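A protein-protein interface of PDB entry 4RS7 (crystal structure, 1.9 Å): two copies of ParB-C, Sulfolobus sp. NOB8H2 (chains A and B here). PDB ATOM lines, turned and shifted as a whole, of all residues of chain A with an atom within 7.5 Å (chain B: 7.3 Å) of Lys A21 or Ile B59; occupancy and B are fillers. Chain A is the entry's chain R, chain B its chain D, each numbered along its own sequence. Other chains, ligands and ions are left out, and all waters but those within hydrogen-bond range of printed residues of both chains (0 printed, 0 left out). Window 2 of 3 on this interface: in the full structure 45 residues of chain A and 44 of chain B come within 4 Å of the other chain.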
ATOM      1  N   LYS A  15       3.262  18.223 -22.456  1.00  0.00           N
ATOM      2  CA  LYS A  15       2.618  16.944 -22.188  1.00  0.00           C
ATOM      3  C   LYS A  15       1.168  16.930 -22.681  1.00  0.00           C
ATOM      4  O   LYS A  15       0.743  15.988 -23.347  1.00  0.00           O
ATOM      5  CB  LYS A  15       2.695  16.613 -20.694  1.00  0.00           C
ATOM      6  CG  LYS A  15       1.928  15.367 -20.278  1.00  0.00           C
ATOM      7  CD  LYS A  15       2.237  15.002 -18.828  1.00  0.00           C
ATOM      8  CE  LYS A  15       1.450  13.780 -18.382  1.00  0.00           C
ATOM      9  NZ  LYS A  15       2.077  13.111 -17.210  1.00  0.00           N
ATOM     10  N   LEU A  16       0.413  17.977 -22.363  1.00  0.00           N
ATOM     11  CA  LEU A  16      -0.981  18.060 -22.789  1.00  0.00           C
ATOM     12  C   LEU A  16      -1.122  17.991 -24.311  1.00  0.00           C
ATOM     13  O   LEU A  16      -2.024  17.335 -24.825  1.00  0.00           O
ATOM     14  CB  LEU A  16      -1.654  19.321 -22.234  1.00  0.00           C
ATOM     15  CG  LEU A  16      -1.930  19.330 -20.725  1.00  0.00           C
ATOM     16  CD1 LEU A  16      -2.442  20.691 -20.260  1.00  0.00           C
ATOM     17  CD2 LEU A  16      -2.912  18.227 -20.339  1.00  0.00           C
ATOM     18  N   VAL A  17      -0.232  18.666 -25.032  1.00  0.00           N
ATOM     19  CA  VAL A  17      -0.245  18.595 -26.492  1.00  0.00           C
ATOM     20  C   VAL A  17       0.112  17.184 -26.972  1.00  0.00           C
ATOM     21  O   VAL A  17      -0.570  16.620 -27.829  1.00  0.00           O
ATOM     22  CB  VAL A  17       0.722  19.612 -27.128  1.00  0.00           C
ATOM     23  CG1 VAL A  17       0.875  19.349 -28.620  1.00  0.00           C
ATOM     24  CG2 VAL A  17       0.247  21.038 -26.873  1.00  0.00           C
ATOM     25  N   ASP A  18       1.176  16.618 -26.406  1.00  0.00           N
ATOM     26  CA  ASP A  18       1.619  15.271 -26.772  1.00  0.00           C
ATOM     27  C   ASP A  18       0.547  14.221 -26.490  1.00  0.00           C
ATOM     28  O   ASP A  18       0.471  13.207 -27.184  1.00  0.00           O
ATOM     29  CB  ASP A  18       2.897  14.894 -26.021  1.00  0.00           C
ATOM     30  CG  ASP A  18       4.108  15.666 -26.500  1.00  0.00           C
ATOM     31  OD1 ASP A  18       4.005  16.355 -27.534  1.00  0.00           O
ATOM     32  OD2 ASP A  18       5.166  15.573 -25.842  1.00  0.00           O
ATOM     33  N   GLU A  19      -0.264  14.467 -25.462  1.00  0.00           N
ATOM     34  CA  GLU A  19      -1.330  13.553 -25.069  1.00  0.00           C
ATOM     35  C   GLU A  19      -2.539  13.712 -25.979  1.00  0.00           C
ATOM     36  O   GLU A  19      -3.477  12.917 -25.927  1.00  0.00           O
ATOM     37  CB  GLU A  19      -1.756  13.804 -23.617  1.00  0.00           C
ATOM     38  CG  GLU A  19      -0.789  13.280 -22.564  1.00  0.00           C
ATOM     39  CD  GLU A  19      -1.287  13.524 -21.148  1.00  0.00           C
ATOM     40  OE1 GLU A  19      -1.960  14.552 -20.919  1.00  0.00           O
ATOM     41  OE2 GLU A  19      -1.015  12.684 -20.265  1.00  0.00           O
ATOM     42  N   GLY A  20      -2.516  14.754 -26.803  1.00  0.00           N
ATOM     43  CA  GLY A  20      -3.605  15.023 -27.721  1.00  0.00           C
ATOM     44  C   GLY A  20      -4.748  15.836 -27.132  1.00  0.00           C
ATOM     45  O   GLY A  20      -5.781  15.989 -27.774  1.00  0.00           O
ATOM     46  N   LYS A  21      -4.569  16.362 -25.922  1.00  0.00           N
ATOM     47  CA  LYS A  21      -5.631  17.124 -25.254  1.00  0.00           C
ATOM     48  C   LYS A  21      -5.635  18.603 -25.640  1.00  0.00           C
ATOM     49  O   LYS A  21      -6.682  19.253 -25.649  1.00  0.00           O
ATOM     50  CB  LYS A  21      -5.525  16.988 -23.731  1.00  0.00           C
ATOM     51  CG  LYS A  21      -5.648  15.562 -23.225  1.00  0.00           C
ATOM     52  CD  LYS A  21      -5.303  15.470 -21.749  1.00  0.00           C
ATOM     53  CE  LYS A  21      -5.248  14.021 -21.285  1.00  0.00           C
ATOM     54  NZ  LYS A  21      -4.603  13.893 -19.945  1.00  0.00           N
ATOM     55  N   LEU A  22      -4.458  19.138 -25.940  1.00  0.00           N
ATOM     56  CA  LEU A  22      -4.354  20.514 -26.404  1.00  0.00           C
ATOM     57  C   LEU A  22      -3.861  20.540 -27.840  1.00  0.00           C
ATOM     58  O   LEU A  22      -2.889  19.867 -28.181  1.00  0.00           O
ATOM     59  CB  LEU A  22      -3.411  21.324 -25.509  1.00  0.00           C
ATOM     60  CG  LEU A  22      -3.974  21.809 -24.173  1.00  0.00           C
ATOM     61  CD1 LEU A  22      -2.902  22.510 -23.347  1.00  0.00           C
ATOM     62  CD2 LEU A  22      -5.166  22.728 -24.404  1.00  0.00           C
ATOM     63  N   THR A  23      -4.535  21.312 -28.683  1.00  0.00           N
ATOM     64  CA  THR A  23      -4.126  21.435 -30.074  1.00  0.00           C
ATOM     65  C   THR A  23      -2.934  22.374 -30.180  1.00  0.00           C
ATOM     66  O   THR A  23      -2.634  23.127 -29.246  1.00  0.00           O
ATOM     67  CB  THR A  23      -5.266  21.970 -30.957  1.00  0.00           C
ATOM     68  OG1 THR A  23      -5.397  23.385 -30.769  1.00  0.00           O
ATOM     69  CG2 THR A  23      -6.584  21.283 -30.609  1.00  0.00           C
ATOM     70  N   ASP A  26      -3.979  25.794 -29.860  1.00  0.00           N
ATOM     71  CA  ASP A  26      -4.149  26.012 -28.429  1.00  0.00           C
ATOM     72  C   ASP A  26      -2.824  26.439 -27.807  1.00  0.00           C
ATOM     73  O   ASP A  26      -2.764  27.419 -27.068  1.00  0.00           O
ATOM     74  CB  ASP A  26      -4.642  24.736 -27.735  1.00  0.00           C
ATOM     75  CG  ASP A  26      -6.119  24.469 -27.966  1.00  0.00           C
ATOM     76  OD1 ASP A  26      -6.861  25.423 -28.280  1.00  0.00           O
ATOM     77  OD2 ASP A  26      -6.539  23.299 -27.816  1.00  0.00           O
ATOM     78  N   ASP B  53      -6.863  29.622 -18.278  1.00  0.00           N
ATOM     79  CA  ASP B  53      -7.728  28.907 -17.345  1.00  0.00           C
ATOM     80  C   ASP B  53      -8.946  28.348 -18.070  1.00  0.00           C
ATOM     81  O   ASP B  53      -9.381  27.230 -17.799  1.00  0.00           O
ATOM     82  CB  ASP B  53      -8.186  29.809 -16.197  1.00  0.00           C
ATOM     83  CG  ASP B  53      -8.844  29.025 -15.072  1.00  0.00           C
ATOM     84  OD1 ASP B  53      -8.277  27.992 -14.667  1.00  0.00           O
ATOM     85  OD2 ASP B  53      -9.923  29.434 -14.594  1.00  0.00           O
ATOM     86  N   LEU B  54      -9.499  29.140 -18.985  1.00  0.00           N
ATOM     87  CA  LEU B  54     -10.690  28.732 -19.724  1.00  0.00           C
ATOM     88  C   LEU B  54     -10.377  27.572 -20.666  1.00  0.00           C
ATOM     89  O   LEU B  54     -11.172  26.642 -20.804  1.00  0.00           O
ATOM     90  CB  LEU B  54     -11.280  29.916 -20.500  1.00  0.00           C
ATOM     91  CG  LEU B  54     -11.759  31.114 -19.674  1.00  0.00           C
ATOM     92  CD1 LEU B  54     -12.278  32.220 -20.589  1.00  0.00           C
ATOM     93  CD2 LEU B  54     -12.822  30.698 -18.662  1.00  0.00           C
ATOM     94  N   LEU B  55      -9.212  27.628 -21.304  1.00  0.00           N
ATOM     95  CA  LEU B  55      -8.773  26.561 -22.199  1.00  0.00           C
ATOM     96  C   LEU B  55      -8.615  25.250 -21.432  1.00  0.00           C
ATOM     97  O   LEU B  55      -9.027  24.190 -21.895  1.00  0.00           O
ATOM     98  CB  LEU B  55      -7.451  26.932 -22.867  1.00  0.00           C
ATOM     99  CG  LEU B  55      -7.336  28.311 -23.512  1.00  0.00           C
ATOM    100  CD1 LEU B  55      -5.878  28.639 -23.806  1.00  0.00           C
ATOM    101  CD2 LEU B  55      -8.176  28.384 -24.776  1.00  0.00           C
ATOM    102  N   LEU B  56      -8.014  25.334 -20.252  1.00  0.00           N
ATOM    103  CA  LEU B  56      -7.749  24.150 -19.442  1.00  0.00           C
ATOM    104  C   LEU B  56      -9.034  23.584 -18.844  1.00  0.00           C
ATOM    105  O   LEU B  56      -9.204  22.368 -18.766  1.00  0.00           O
ATOM    106  CB  LEU B  56      -6.723  24.453 -18.346  1.00  0.00           C
ATOM    107  CG  LEU B  56      -5.338  24.864 -18.847  1.00  0.00           C
ATOM    108  CD1 LEU B  56      -4.412  25.167 -17.676  1.00  0.00           C
ATOM    109  CD2 LEU B  56      -4.750  23.779 -19.748  1.00  0.00           C
ATOM    110  N   LYS B  57      -9.938  24.464 -18.426  1.00  0.00           N
ATOM    111  CA  LYS B  57     -11.240  24.035 -17.928  1.00  0.00           C
ATOM    112  C   LYS B  57     -11.966  23.249 -19.003  1.00  0.00           C
ATOM    113  O   LYS B  57     -12.538  22.196 -18.742  1.00  0.00           O
ATOM    114  CB  LYS B  57     -12.080  25.245 -17.502  1.00  0.00           C
ATOM    115  CG  LYS B  57     -11.680  25.832 -16.168  1.00  0.00           C
ATOM    116  CD  LYS B  57     -12.270  27.217 -15.933  1.00  0.00           C
ATOM    117  CE  LYS B  57     -13.760  27.176 -15.629  1.00  0.00           C
ATOM    118  NZ  LYS B  57     -14.264  28.525 -15.222  1.00  0.00           N
ATOM    119  N   ARG B  58     -11.920  23.781 -20.219  1.00  0.00           N
ATOM    120  CA  ARG B  58     -12.594  23.190 -21.367  1.00  0.00           C
ATOM    121  C   ARG B  58     -12.144  21.757 -21.635  1.00  0.00           C
ATOM    122  O   ARG B  58     -12.945  20.930 -22.069  1.00  0.00           O
ATOM    123  CB  ARG B  58     -12.388  24.050 -22.621  1.00  0.00           C
ATOM    124  CG  ARG B  58     -12.908  23.421 -23.901  1.00  0.00           C
ATOM    125  CD  ARG B  58     -12.686  24.324 -25.110  1.00  0.00           C
ATOM    126  NE  ARG B  58     -11.843  23.679 -26.114  1.00  0.00           N
ATOM    127  CZ  ARG B  58     -10.596  24.045 -26.394  1.00  0.00           C
ATOM    128  NH1 ARG B  58     -10.036  25.065 -25.755  1.00  0.00           N
ATOM    129  NH2 ARG B  58      -9.909  23.396 -27.325  1.00  0.00           N
ATOM    130  N   ILE B  59     -10.877  21.452 -21.371  1.00  0.00           N
ATOM    131  CA  ILE B  59     -10.375  20.102 -21.622  1.00  0.00           C
ATOM    132  C   ILE B  59     -10.403  19.222 -20.372  1.00  0.00           C
ATOM    133  O   ILE B  59      -9.831  18.133 -20.358  1.00  0.00           O
ATOM    134  CB  ILE B  59      -8.968  20.095 -22.272  1.00  0.00           C
ATOM    135  CG1 ILE B  59      -7.923  20.685 -21.325  1.00  0.00           C
ATOM    136  CG2 ILE B  59      -8.984  20.848 -23.593  1.00  0.00           C
ATOM    137  CD1 ILE B  59      -6.502  20.564 -21.848  1.00  0.00           C
ATOM    138  N   GLY B  60     -11.066  19.704 -19.325  1.00  0.00           N
ATOM    139  CA  GLY B  60     -11.393  18.869 -18.183  1.00  0.00           C
ATOM    140  C   GLY B  60     -10.513  18.963 -16.951  1.00  0.00           C
ATOM    141  O   GLY B  60     -10.787  18.305 -15.948  1.00  0.00           O
ATOM    142  N   LEU B  61      -9.461  19.773 -17.006  1.00  0.00           N
ATOM    143  CA  LEU B  61      -8.546  19.872 -15.868  1.00  0.00           C
ATOM    144  C   LEU B  61      -9.234  20.369 -14.598  1.00  0.00           C
ATOM    145  O   LEU B  61     -10.099  21.243 -14.644  1.00  0.00           O
ATOM    146  CB  LEU B  61      -7.335  20.750 -16.201  1.00  0.00           C
ATOM    147  CG  LEU B  61      -6.154  20.056 -16.887  1.00  0.00           C
ATOM    148  CD1 LEU B  61      -6.543  19.533 -18.262  1.00  0.00           C
ATOM    149  CD2 LEU B  61      -4.965  21.001 -16.991  1.00  0.00           C
ATOM    150  N   SER B  62      -8.843  19.797 -13.463  1.00  0.00           N
ATOM    151  CA  SER B  62      -9.374  20.208 -12.174  1.00  0.00           C
ATOM    152  C   SER B  62      -8.776  21.544 -11.761  1.00  0.00           C
ATOM    153  O   SER B  62      -7.830  22.030 -12.386  1.00  0.00           O
ATOM    154  CB  SER B  62      -9.058  19.160 -11.109  1.00  0.00           C
ATOM    155  OG  SER B  62      -7.673  19.145 -10.810  1.00  0.00           O
ATOM    156  N   ILE B  69      -0.444  24.628 -13.273  1.00  0.00           N
ATOM    157  CA  ILE B  69       0.044  25.126 -14.555  1.00  0.00           C
ATOM    158  C   ILE B  69       0.315  26.631 -14.496  1.00  0.00           C
ATOM    159  O   ILE B  69       1.300  27.108 -15.058  1.00  0.00           O
ATOM    160  CB  ILE B  69      -0.898  24.744 -15.725  1.00  0.00           C
ATOM    161  CG1 ILE B  69      -0.908  23.220 -15.898  1.00  0.00           C
ATOM    162  CG2 ILE B  69      -0.449  25.409 -17.032  1.00  0.00           C
ATOM    163  CD1 ILE B  69      -1.724  22.727 -17.067  1.00  0.00           C
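Of the printed residues of chain B, Leu A16 touches Leu B56 and Ile B69. Val A17 touches none of the printed residues of chain B. No residue of chain B comes within 4 Å of Gly A20. Lys A21 touches one residue of chain B. Of the printed residues of chain B, Leu A22 touches Ile B59 (3.6 Å). Ile B59 touches just these residues of chain A: Lys A21 (3.5 Å) and Leu A22 (3.6 Å). The nearest printed residue of chain B that does not touch Lys A21 is Leu B61 (5.5 Å).
Leu A16 touches Leu B56 (CD1 to CD2, 3.9 Å). CD1 of Leu A16 touches CD1 of Ile B69 (3.9 Å). Ile B59 touches Lys A21. Leu A22 touches Ile B59 (CD2 to CD1, 3.6 Å).
The backbone carbonyl oxygen (O) of Leu B56 is in hydrogen-bond range of the backbone NH (N) of Leu B61 (3.1 Å). The backbone carbonyl oxygen of Leu A16 sits at hydrogen-bond distance from the backbone NH of Leu A22, 3.2 Å away. N of Lys A21 sits at hydrogen-bond distance from O of Leu A16, at 2.9 Å. OE1 of Glu A19 is in salt-bridge range of NZ of Lys A21. The side-chain hydroxyl (OG1) of Thr A23 is in hydrogen-bond range of the backbone NH (N) of Asp A26, 2.9 Å away.
Of the 11 printed residues of chain B, 4 touch a printed residue of chain A. Printed residues of chain B that touch a printed residue of chain A: Leu B56, Arg B58, Ile B59 and Ile B69. Of the 10 printed residues of chain A, 4 touch a printed residue of chain B. Hydrophobic or aromatic side chains of chain A that line the printed part of chain B: Leu A16 and Leu A22. Among the printed residues, Asp or Glu carboxylates within 4 Å of a Lys or Arg side-chain nitrogen of the other chain: Asp A26 with Arg B58.
No position is printed for both chains. Of the 5 pairs that touch across the chains among the printed residues, none has its exchanged pair printed and touching as well.
NH2 of Arg B58 is in salt-bridge range of OD2 of Asp A26 (3.4 Å).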
